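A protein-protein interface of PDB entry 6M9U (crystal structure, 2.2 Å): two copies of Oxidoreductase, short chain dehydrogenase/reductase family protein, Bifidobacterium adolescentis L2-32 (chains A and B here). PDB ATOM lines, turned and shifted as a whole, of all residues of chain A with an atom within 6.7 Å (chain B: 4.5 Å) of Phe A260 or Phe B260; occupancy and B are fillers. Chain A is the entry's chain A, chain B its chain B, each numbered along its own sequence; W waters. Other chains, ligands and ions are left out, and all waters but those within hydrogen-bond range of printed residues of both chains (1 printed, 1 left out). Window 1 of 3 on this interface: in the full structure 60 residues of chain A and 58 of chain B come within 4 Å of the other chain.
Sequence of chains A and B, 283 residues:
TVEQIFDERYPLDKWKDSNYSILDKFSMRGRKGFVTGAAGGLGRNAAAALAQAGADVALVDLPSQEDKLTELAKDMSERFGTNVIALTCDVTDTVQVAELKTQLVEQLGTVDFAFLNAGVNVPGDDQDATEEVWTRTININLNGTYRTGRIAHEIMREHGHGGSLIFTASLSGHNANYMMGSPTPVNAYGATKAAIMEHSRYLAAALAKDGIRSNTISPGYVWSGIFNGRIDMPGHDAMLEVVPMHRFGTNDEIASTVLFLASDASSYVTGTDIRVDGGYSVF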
ATOM      1  N   LYS A  25     -18.622  26.392   0.020  1.00  0.00           N
ATOM      2  CA  LYS A  25     -19.404  25.320  -0.584  1.00  0.00           C
ATOM      3  C   LYS A  25     -19.988  24.400   0.491  1.00  0.00           C
ATOM      4  O   LYS A  25     -21.058  23.805   0.304  1.00  0.00           O
ATOM      5  CB  LYS A  25     -18.534  24.535  -1.565  1.00  0.00           C
ATOM      6  CG  LYS A  25     -18.439  25.126  -2.976  1.00  0.00           C
ATOM      7  CD  LYS A  25     -17.443  24.250  -3.833  1.00  0.00           C
ATOM      8  CE  LYS A  25     -17.249  24.700  -5.305  1.00  0.00           C
ATOM      9  NZ  LYS A  25     -18.387  24.224  -6.115  1.00  0.00           N
ATOM     10  N   PHE A  26     -19.313  24.285   1.614  1.00  0.00           N
ATOM     11  CA  PHE A  26     -19.766  23.364   2.627  1.00  0.00           C
ATOM     12  C   PHE A  26     -20.721  23.996   3.626  1.00  0.00           C
ATOM     13  O   PHE A  26     -21.272  23.286   4.466  1.00  0.00           O
ATOM     14  CB  PHE A  26     -18.590  22.784   3.353  1.00  0.00           C
ATOM     15  CG  PHE A  26     -17.679  21.982   2.475  1.00  0.00           C
ATOM     16  CD1 PHE A  26     -16.790  22.607   1.638  1.00  0.00           C
ATOM     17  CD2 PHE A  26     -17.726  20.588   2.495  1.00  0.00           C
ATOM     18  CE1 PHE A  26     -15.952  21.872   0.831  1.00  0.00           C
ATOM     19  CE2 PHE A  26     -16.877  19.846   1.692  1.00  0.00           C
ATOM     20  CZ  PHE A  26     -15.979  20.486   0.868  1.00  0.00           C
ATOM     21  N   LEU A  50     -26.052  19.556   9.940  1.00  0.00           N
ATOM     22  CA  LEU A  50     -26.633  20.507   9.015  1.00  0.00           C
ATOM     23  C   LEU A  50     -26.910  21.824   9.708  1.00  0.00           C
ATOM     24  O   LEU A  50     -26.709  22.898   9.127  1.00  0.00           O
ATOM     25  CB  LEU A  50     -27.901  19.901   8.390  1.00  0.00           C
ATOM     26  CG  LEU A  50     -27.626  18.711   7.454  1.00  0.00           C
ATOM     27  CD1 LEU A  50     -28.814  17.795   7.211  1.00  0.00           C
ATOM     28  CD2 LEU A  50     -27.142  19.239   6.122  1.00  0.00           C
ATOM     29  N   SER A 164     -31.495  18.955  -2.725  1.00  0.00           N
ATOM     30  CA  SER A 164     -30.669  17.761  -2.618  1.00  0.00           C
ATOM     31  C   SER A 164     -31.386  16.752  -1.743  1.00  0.00           C
ATOM     32  O   SER A 164     -31.780  17.100  -0.637  1.00  0.00           O
ATOM     33  CB  SER A 164     -29.301  18.106  -2.023  1.00  0.00           C
ATOM     34  OG  SER A 164     -28.502  16.957  -1.904  1.00  0.00           O
ATOM     35  N   ARG A 213     -30.823  16.994  -6.921  1.00  0.00           N
ATOM     36  CA  ARG A 213     -29.923  15.847  -6.859  1.00  0.00           C
ATOM     37  C   ARG A 213     -30.490  14.807  -5.885  1.00  0.00           C
ATOM     38  O   ARG A 213     -31.251  15.121  -4.972  1.00  0.00           O
ATOM     39  CB  ARG A 213     -28.519  16.285  -6.442  1.00  0.00           C
ATOM     40  CG  ARG A 213     -27.948  17.383  -7.337  1.00  0.00           C
ATOM     41  CD  ARG A 213     -26.528  17.762  -6.969  1.00  0.00           C
ATOM     42  NE  ARG A 213     -26.394  18.568  -5.746  1.00  0.00           N
ATOM     43  CZ  ARG A 213     -25.892  18.112  -4.598  1.00  0.00           C
ATOM     44  NH1 ARG A 213     -25.495  16.849  -4.468  1.00  0.00           N
ATOM     45  NH2 ARG A 213     -25.805  18.925  -3.557  1.00  0.00           N
ATOM     46  N   GLU A 253     -19.549  10.415  11.664  1.00  0.00           N
ATOM     47  CA  GLU A 253     -18.867  10.058  10.419  1.00  0.00           C
ATOM     48  C   GLU A 253     -19.830   9.848   9.259  1.00  0.00           C
ATOM     49  O   GLU A 253     -19.434   9.980   8.100  1.00  0.00           O
ATOM     50  CB  GLU A 253     -18.004   8.816  10.666  1.00  0.00           C
ATOM     51  CG  GLU A 253     -16.806   9.132  11.581  1.00  0.00           C
ATOM     52  CD  GLU A 253     -15.854   7.950  11.834  1.00  0.00           C
ATOM     53  OE1 GLU A 253     -16.300   6.901  12.367  1.00  0.00           O
ATOM     54  OE2 GLU A 253     -14.639   8.084  11.488  1.00  0.00           O
ATOM     55  N   ALA A 255     -22.795  11.737   9.517  1.00  0.00           N
ATOM     56  CA  ALA A 255     -23.308  13.095   9.419  1.00  0.00           C
ATOM     57  C   ALA A 255     -22.470  13.953   8.468  1.00  0.00           C
ATOM     58  O   ALA A 255     -23.009  14.790   7.726  1.00  0.00           O
ATOM     59  CB  ALA A 255     -23.334  13.758  10.808  1.00  0.00           C
ATOM     60  N   SER A 256     -21.132  13.834   8.531  1.00  0.00           N
ATOM     61  CA  SER A 256     -20.337  14.683   7.659  1.00  0.00           C
ATOM     62  C   SER A 256     -20.537  14.323   6.186  1.00  0.00           C
ATOM     63  O   SER A 256     -20.472  15.206   5.321  1.00  0.00           O
ATOM     64  CB  SER A 256     -18.841  14.603   7.993  1.00  0.00           C
ATOM     65  OG  SER A 256     -18.379  13.277   8.059  1.00  0.00           O
ATOM     66  N   THR A 257     -20.779  13.052   5.882  1.00  0.00           N
ATOM     67  CA  THR A 257     -21.098  12.688   4.504  1.00  0.00           C
ATOM     68  C   THR A 257     -22.458  13.243   4.106  1.00  0.00           C
ATOM     69  O   THR A 257     -22.635  13.728   2.983  1.00  0.00           O
ATOM     70  CB  THR A 257     -21.059  11.175   4.340  1.00  0.00           C
ATOM     71  OG1 THR A 257     -19.804  10.683   4.821  1.00  0.00           O
ATOM     72  CG2 THR A 257     -21.187  10.767   2.883  1.00  0.00           C
ATOM     73  N   VAL A 258     -23.423  13.209   5.027  1.00  0.00           N
ATOM     74  CA  VAL A 258     -24.716  13.817   4.740  1.00  0.00           C
ATOM     75  C   VAL A 258     -24.538  15.280   4.385  1.00  0.00           C
ATOM     76  O   VAL A 258     -25.205  15.808   3.477  1.00  0.00           O
ATOM     77  CB  VAL A 258     -25.682  13.663   5.926  1.00  0.00           C
ATOM     78  CG1 VAL A 258     -26.978  14.462   5.619  1.00  0.00           C
ATOM     79  CG2 VAL A 258     -26.034  12.217   6.184  1.00  0.00           C
ATOM     80  N   LEU A 259     -23.675  15.977   5.136  1.00  0.00           N
ATOM     81  CA  LEU A 259     -23.448  17.402   4.884  1.00  0.00           C
ATOM     82  C   LEU A 259     -22.782  17.617   3.530  1.00  0.00           C
ATOM     83  O   LEU A 259     -23.095  18.574   2.782  1.00  0.00           O
ATOM     84  CB  LEU A 259     -22.568  17.996   5.986  1.00  0.00           C
ATOM     85  CG  LEU A 259     -22.155  19.448   5.771  1.00  0.00           C
ATOM     86  CD1 LEU A 259     -23.381  20.352   5.660  1.00  0.00           C
ATOM     87  CD2 LEU A 259     -21.296  19.847   6.942  1.00  0.00           C
ATOM     88  N   PHE A 260     -21.825  16.765   3.194  1.00  0.00           N
ATOM     89  CA  PHE A 260     -21.208  16.888   1.872  1.00  0.00           C
ATOM     90  C   PHE A 260     -22.279  16.784   0.771  1.00  0.00           C
ATOM     91  O   PHE A 260     -22.349  17.640  -0.125  1.00  0.00           O
ATOM     92  CB  PHE A 260     -20.086  15.843   1.745  1.00  0.00           C
ATOM     93  CG  PHE A 260     -19.551  15.691   0.358  1.00  0.00           C
ATOM     94  CD1 PHE A 260     -18.755  16.694  -0.215  1.00  0.00           C
ATOM     95  CD2 PHE A 260     -19.806  14.542  -0.386  1.00  0.00           C
ATOM     96  CE1 PHE A 260     -18.240  16.546  -1.506  1.00  0.00           C
ATOM     97  CE2 PHE A 260     -19.301  14.408  -1.711  1.00  0.00           C
ATOM     98  CZ  PHE A 260     -18.529  15.412  -2.249  1.00  0.00           C
ATOM     99  N   LEU A 261     -23.180  15.783   0.861  1.00  0.00           N
ATOM    100  CA  LEU A 261     -24.174  15.585  -0.198  1.00  0.00           C
ATOM    101  C   LEU A 261     -25.239  16.670  -0.197  1.00  0.00           C
ATOM    102  O   LEU A 261     -25.806  16.985  -1.265  1.00  0.00           O
ATOM    103  CB  LEU A 261     -24.839  14.209  -0.064  1.00  0.00           C
ATOM    104  CG  LEU A 261     -23.838  13.077  -0.369  1.00  0.00           C
ATOM    105  CD1 LEU A 261     -24.339  11.704   0.029  1.00  0.00           C
ATOM    106  CD2 LEU A 261     -23.422  13.104  -1.834  1.00  0.00           C
ATOM    107  N   ALA A 262     -25.507  17.263   0.966  1.00  0.00           N
ATOM    108  CA  ALA A 262     -26.537  18.285   1.038  1.00  0.00           C
ATOM    109  C   ALA A 262     -26.053  19.631   0.528  1.00  0.00           C
ATOM    110  O   ALA A 262     -26.861  20.441   0.053  1.00  0.00           O
ATOM    111  CB  ALA A 262     -27.045  18.407   2.474  1.00  0.00           C
ATOM    112  N   SER A 263     -24.747  19.892   0.609  1.00  0.00           N
ATOM    113  CA  SER A 263     -24.208  21.202   0.309  1.00  0.00           C
ATOM    114  C   SER A 263     -23.766  21.300  -1.135  1.00  0.00           C
ATOM    115  O   SER A 263     -23.615  20.287  -1.822  1.00  0.00           O
ATOM    116  CB  SER A 263     -23.008  21.472   1.221  1.00  0.00           C
ATOM    117  OG  SER A 263     -21.853  20.702   0.801  1.00  0.00           O
ATOM    118  N   ASP A 264     -23.449  22.535  -1.561  1.00  0.00           N
ATOM    119  CA  ASP A 264     -22.878  22.789  -2.879  1.00  0.00           C
ATOM    120  C   ASP A 264     -21.523  22.146  -3.099  1.00  0.00           C
ATOM    121  O   ASP A 264     -21.055  22.111  -4.235  1.00  0.00           O
ATOM    122  CB  ASP A 264     -22.747  24.296  -3.109  1.00  0.00           C
ATOM    123  CG  ASP A 264     -24.093  24.977  -3.160  1.00  0.00           C
ATOM    124  OD1 ASP A 264     -25.084  24.236  -3.024  1.00  0.00           O
ATOM    125  OD2 ASP A 264     -24.172  26.221  -3.317  1.00  0.00           O
ATOM    126  N   ALA A 265     -20.896  21.594  -2.081  1.00  0.00           N
ATOM    127  CA  ALA A 265     -19.645  20.884  -2.337  1.00  0.00           C
ATOM    128  C   ALA A 265     -19.835  19.689  -3.268  1.00  0.00           C
ATOM    129  O   ALA A 265     -18.872  19.214  -3.850  1.00  0.00           O
ATOM    130  CB  ALA A 265     -19.036  20.396  -1.023  1.00  0.00           C
ATOM    131  N   SER A 266     -21.039  19.149  -3.363  1.00  0.00           N
ATOM    132  CA  SER A 266     -21.329  17.956  -4.143  1.00  0.00           C
ATOM    133  C   SER A 266     -22.266  18.292  -5.284  1.00  0.00           C
ATOM    134  O   SER A 266     -23.091  17.468  -5.663  1.00  0.00           O
ATOM    135  CB  SER A 266     -21.923  16.879  -3.233  1.00  0.00           C
ATOM    136  OG  SER A 266     -23.186  17.296  -2.776  1.00  0.00           O
ATOM    137  N   SER A 267     -22.157  19.529  -5.829  1.00  0.00           N
ATOM    138  CA  SER A 267     -23.115  20.070  -6.799  1.00  0.00           C
ATOM    139  C   SER A 267     -23.136  19.326  -8.146  1.00  0.00           C
ATOM    140  O   SER A 267     -24.138  19.393  -8.859  1.00  0.00           O
ATOM    141  CB  SER A 267     -22.816  21.560  -7.034  1.00  0.00           C
ATOM    142  OG  SER A 267     -21.488  21.785  -7.461  1.00  0.00           O
ATOM    143  N   VAL A 269     -22.714  16.008  -8.125  1.00  0.00           N
ATOM    144  CA  VAL A 269     -22.852  14.618  -7.680  1.00  0.00           C
ATOM    145  C   VAL A 269     -24.327  14.273  -7.623  1.00  0.00           C
ATOM    146  O   VAL A 269     -25.066  14.833  -6.806  1.00  0.00           O
ATOM    147  CB  VAL A 269     -22.188  14.368  -6.323  1.00  0.00           C
ATOM    148  CG1 VAL A 269     -22.354  12.922  -5.906  1.00  0.00           C
ATOM    149  CG2 VAL A 269     -20.734  14.771  -6.379  1.00  0.00           C
ATOM    150  N   ILE A 274     -22.433   6.903  -1.630  1.00  0.00           N
ATOM    151  CA  ILE A 274     -21.193   6.998  -0.882  1.00  0.00           C
ATOM    152  C   ILE A 274     -21.227   5.965   0.221  1.00  0.00           C
ATOM    153  O   ILE A 274     -22.079   6.020   1.104  1.00  0.00           O
ATOM    154  CB  ILE A 274     -20.935   8.402  -0.313  1.00  0.00           C
ATOM    155  CG1 ILE A 274     -20.951   9.400  -1.473  1.00  0.00           C
ATOM    156  CG2 ILE A 274     -19.596   8.446   0.409  1.00  0.00           C
ATOM    157  CD1 ILE A 274     -20.572  10.812  -1.126  1.00  0.00           C
ATOM    158  N   VAL A 276     -19.680   4.293   3.522  1.00  0.00           N
ATOM    159  CA  VAL A 276     -19.023   4.822   4.717  1.00  0.00           C
ATOM    160  C   VAL A 276     -18.942   3.659   5.679  1.00  0.00           C
ATOM    161  O   VAL A 276     -19.767   3.540   6.569  1.00  0.00           O
ATOM    162  CB  VAL A 276     -19.789   5.998   5.309  1.00  0.00           C
ATOM    163  CG1 VAL A 276     -19.033   6.605   6.481  1.00  0.00           C
ATOM    164  CG2 VAL A 276     -20.047   7.051   4.255  1.00  0.00           C
ATOM    165  N   PHE B  26     -13.625  19.512   7.716  1.00  0.00           N
ATOM    166  CA  PHE B  26     -13.222  19.761   6.337  1.00  0.00           C
ATOM    167  C   PHE B  26     -11.984  20.645   6.232  1.00  0.00           C
ATOM    168  O   PHE B  26     -11.560  20.971   5.126  1.00  0.00           O
ATOM    169  CB  PHE B  26     -14.397  20.418   5.599  1.00  0.00           C
ATOM    170  CG  PHE B  26     -15.657  19.586   5.601  1.00  0.00           C
ATOM    171  CD1 PHE B  26     -16.550  19.646   6.643  1.00  0.00           C
ATOM    172  CD2 PHE B  26     -15.946  18.734   4.539  1.00  0.00           C
ATOM    173  CE1 PHE B  26     -17.711  18.883   6.644  1.00  0.00           C
ATOM    174  CE2 PHE B  26     -17.087  17.967   4.527  1.00  0.00           C
ATOM    175  CZ  PHE B  26     -17.979  18.033   5.589  1.00  0.00           C
ATOM    176  N   SER B 256     -13.757  20.162  -4.670  1.00  0.00           N
ATOM    177  CA  SER B 256     -14.467  20.048  -3.403  1.00  0.00           C
ATOM    178  C   SER B 256     -14.584  18.596  -2.961  1.00  0.00           C
ATOM    179  O   SER B 256     -14.573  18.314  -1.755  1.00  0.00           O
ATOM    180  CB  SER B 256     -15.821  20.734  -3.521  1.00  0.00           C
ATOM    181  OG  SER B 256     -16.626  20.134  -4.495  1.00  0.00           O
ATOM    182  N   THR B 257     -14.650  17.647  -3.921  1.00  0.00           N
ATOM    183  CA  THR B 257     -14.709  16.216  -3.580  1.00  0.00           C
ATOM    184  C   THR B 257     -13.358  15.672  -3.110  1.00  0.00           C
ATOM    185  O   THR B 257     -13.301  14.804  -2.228  1.00  0.00           O
ATOM    186  CB  THR B 257     -15.242  15.424  -4.792  1.00  0.00           C
ATOM    187  OG1 THR B 257     -16.532  15.919  -5.203  1.00  0.00           O
ATOM    188  CG2 THR B 257     -15.368  13.939  -4.452  1.00  0.00           C
ATOM    189  N   VAL B 258     -12.272  16.190  -3.671  1.00  0.00           N
ATOM    190  CA  VAL B 258     -10.934  15.873  -3.173  1.00  0.00           C
ATOM    191  C   VAL B 258     -10.776  16.343  -1.730  1.00  0.00           C
ATOM    192  O   VAL B 258     -10.201  15.642  -0.897  1.00  0.00           O
ATOM    193  CB  VAL B 258      -9.859  16.513  -4.094  1.00  0.00           C
ATOM    194  CG1 VAL B 258      -8.446  16.255  -3.537  1.00  0.00           C
ATOM    195  CG2 VAL B 258      -9.983  15.996  -5.531  1.00  0.00           C
ATOM    196  N   LEU B 259     -11.230  17.559  -1.438  1.00  0.00           N
ATOM    197  CA  LEU B 259     -11.151  18.083  -0.082  1.00  0.00           C
ATOM    198  C   LEU B 259     -11.949  17.229   0.917  1.00  0.00           C
ATOM    199  O   LEU B 259     -11.459  16.893   2.010  1.00  0.00           O
ATOM    200  CB  LEU B 259     -11.631  19.525  -0.079  1.00  0.00           C
ATOM    201  CG  LEU B 259     -11.637  20.134   1.329  1.00  0.00           C
ATOM    202  CD1 LEU B 259     -10.273  20.108   2.009  1.00  0.00           C
ATOM    203  CD2 LEU B 259     -12.124  21.535   1.141  1.00  0.00           C
ATOM    204  N   PHE B 260     -13.141  16.806   0.537  1.00  0.00           N
ATOM    205  CA  PHE B 260     -13.860  15.858   1.365  1.00  0.00           C
ATOM    206  C   PHE B 260     -13.026  14.627   1.685  1.00  0.00           C
ATOM    207  O   PHE B 260     -12.902  14.217   2.855  1.00  0.00           O
ATOM    208  CB  PHE B 260     -15.163  15.448   0.668  1.00  0.00           C
ATOM    209  CG  PHE B 260     -15.943  14.396   1.397  1.00  0.00           C
ATOM    210  CD1 PHE B 260     -16.446  14.639   2.656  1.00  0.00           C
ATOM    211  CD2 PHE B 260     -16.187  13.188   0.807  1.00  0.00           C
ATOM    212  CE1 PHE B 260     -17.186  13.679   3.310  1.00  0.00           C
ATOM    213  CE2 PHE B 260     -16.939  12.213   1.454  1.00  0.00           C
ATOM    214  CZ  PHE B 260     -17.427  12.460   2.707  1.00  0.00           C
ATOM    215  N   LEU B 261     -12.452  14.008   0.649  1.00  0.00           N
ATOM    216  CA  LEU B 261     -11.786  12.719   0.860  1.00  0.00           C
ATOM    217  C   LEU B 261     -10.456  12.886   1.543  1.00  0.00           C
ATOM    218  O   LEU B 261     -10.005  11.961   2.224  1.00  0.00           O
ATOM    219  CB  LEU B 261     -11.588  11.976  -0.450  1.00  0.00           C
ATOM    220  CG  LEU B 261     -12.876  11.473  -1.066  1.00  0.00           C
ATOM    221  CD1 LEU B 261     -12.633  10.954  -2.448  1.00  0.00           C
ATOM    222  CD2 LEU B 261     -13.497  10.382  -0.168  1.00  0.00           C
ATOM    223  N   ALA B 262      -9.783  14.046   1.356  1.00  0.00           N
ATOM    224  CA  ALA B 262      -8.509  14.289   2.018  1.00  0.00           C
ATOM    225  C   ALA B 262      -8.695  14.717   3.468  1.00  0.00           C
ATOM    226  O   ALA B 262      -7.832  14.446   4.299  1.00  0.00           O
ATOM    227  CB  ALA B 262      -7.755  15.367   1.286  1.00  0.00           C
ATOM    228  N   SER B 263      -9.821  15.348   3.815  1.00  0.00           N
ATOM    229  CA  SER B 263     -10.073  15.863   5.151  1.00  0.00           C
ATOM    230  C   SER B 263     -10.599  14.776   6.093  1.00  0.00           C
ATOM    231  O   SER B 263     -10.979  13.684   5.686  1.00  0.00           O
ATOM    232  CB  SER B 263     -11.124  16.971   5.096  1.00  0.00           C
ATOM    233  OG  SER B 263     -12.431  16.387   4.876  1.00  0.00           O
ATOM    234  N   ALA B 265     -13.350  14.853   7.511  1.00  0.00           N
ATOM    235  CA  ALA B 265     -14.766  14.643   7.257  1.00  0.00           C
ATOM    236  C   ALA B 265     -15.046  13.248   6.729  1.00  0.00           C
ATOM    237  O   ALA B 265     -16.129  12.685   6.965  1.00  0.00           O
ATOM    238  CB  ALA B 265     -15.279  15.682   6.262  1.00  0.00           C
ATOM    239  N   SER B 266     -14.106  12.668   5.995  1.00  0.00           N
ATOM    240  CA  SER B 266     -14.330  11.358   5.375  1.00  0.00           C
ATOM    241  C   SER B 266     -13.600  10.270   6.124  1.00  0.00           C
ATOM    242  O   SER B 266     -13.231   9.250   5.537  1.00  0.00           O
ATOM    243  CB  SER B 266     -13.899  11.378   3.900  1.00  0.00           C
ATOM    244  OG  SER B 266     -12.501  11.678   3.771  1.00  0.00           O
ATOM    245  N   ILE B 274     -16.134   7.967  -5.428  1.00  0.00           N
ATOM    246  CA  ILE B 274     -17.174   8.975  -5.559  1.00  0.00           C
ATOM    247  C   ILE B 274     -17.281   9.351  -7.036  1.00  0.00           C
ATOM    248  O   ILE B 274     -16.323   9.880  -7.607  1.00  0.00           O
ATOM    249  CB  ILE B 274     -16.891  10.198  -4.672  1.00  0.00           C
ATOM    250  CG1 ILE B 274     -16.763   9.756  -3.224  1.00  0.00           C
ATOM    251  CG2 ILE B 274     -18.057  11.207  -4.787  1.00  0.00           C
ATOM    252  CD1 ILE B 274     -16.698  10.889  -2.197  1.00  0.00           C
HETATM  253  O   HOH W   1     -16.518   9.648   7.512  1.00  0.00           O
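OG of Ser A256 sits at hydrogen-bond distance from O of Ala B265, 2.6 Å away.
The backbone carbonyl oxygen (O) of Ala A265 lies within hydrogen-bond range of the side-chain hydroxyl (OG) of Ser B256.
The backbone carbonyl oxygen of Phe A260 sits at hydrogen-bond distance from the side-chain hydroxyl of Ser A266.
The backbone carbonyl oxygen (O) of Lys A25 sits at hydrogen-bond distance from the backbone NH (N) of Asp A264, at 3.3 Å.
The side-chain hydroxyl of Ser A263 is in hydrogen-bond range of the backbone carbonyl oxygen of Phe A260 (3.2 Å).
The backbone carbonyl oxygen (O) of Phe B260 sits at hydrogen-bond distance from the side-chain hydroxyl (OG) of Ser B266 (2.7 Å).
The side-chain hydroxyl (OG1) of Thr A257 lies within hydrogen-bond range of the backbone carbonyl oxygen (O) of Glu A253, at 3.4 Å.
OG of Ser B263 sits at hydrogen-bond distance from O of Phe B260 (3.0 Å).
Among the printed residues, merely in contact across the chains: Phe A26 with Phe B26 (3.2 Å), Phe A260 with Thr B257 (3.6 Å), Thr A257 with Phe B260 (3.6 Å), Phe A26 with Ser B256 (3.7 Å), Leu A259 with Phe B26 (3.7 Å), Ser A256 with Phe B26 (3.8 Å), Phe A26 with Leu B259 (3.9 Å), Lys A25 with Ser B256 (3.9 Å) and Phe A260 with Phe B260 (3.9 Å).
Of chain A, only Thr A257 and Phe A260 come within 4 Å of Phe B260.
Of the printed residues of chain B, Lys A25 touches Ser B256.
Printed residues of chain A within 4 Å of Thr B257: Phe A260 (3.6 Å).
Printed residues of chain A within 4 Å of Phe B26: Phe A26 (3.2 Å), Ser A256 (3.8 Å) and Leu A259 (3.7 Å).
Of the printed residues of chain B, Ala A265 touches Ser B256 (2.5 Å).
Printed residues of chain B within 4 Å of Leu A259: Phe B26 (3.7 Å).
Ser B266 touches none of the printed residues of chain A.
Hydrophobic or aromatic side chains of chain B within 4 Å of the printed part of chain A: Phe B26, Leu B259 and Phe B260.
Of the 22 printed residues of chain A, 7 touch a printed residue of chain B.
Among the printed residues, 11 pairs touch across the chains.
Among the printed residues, no Asp or Glu carboxylate lies within 4 Å of a Lys or Arg side-chain nitrogen of the other chain.
Phe B26 touches its own counterpart, Phe A26.
Phe A26 touches Ser B256, and with the chains exchanged Ser A256 touches Phe B26.
Phe A26 touches Leu B259, and with the chains exchanged Leu A259 touches Phe B26.
Thr A257 touches Phe B260, and with the chains exchanged Phe A260 touches Thr B257.
Of the 11 pairs that touch across the chains among the printed residues, 10 have their exchanged pair printed and touching as well.
Water W1 lies within hydrogen-bond range of the backbone carbonyl oxygen (O) of Glu A253 (3.0 Å) and the backbone carbonyl oxygen (O) of Ala B265 (3.1 Å).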
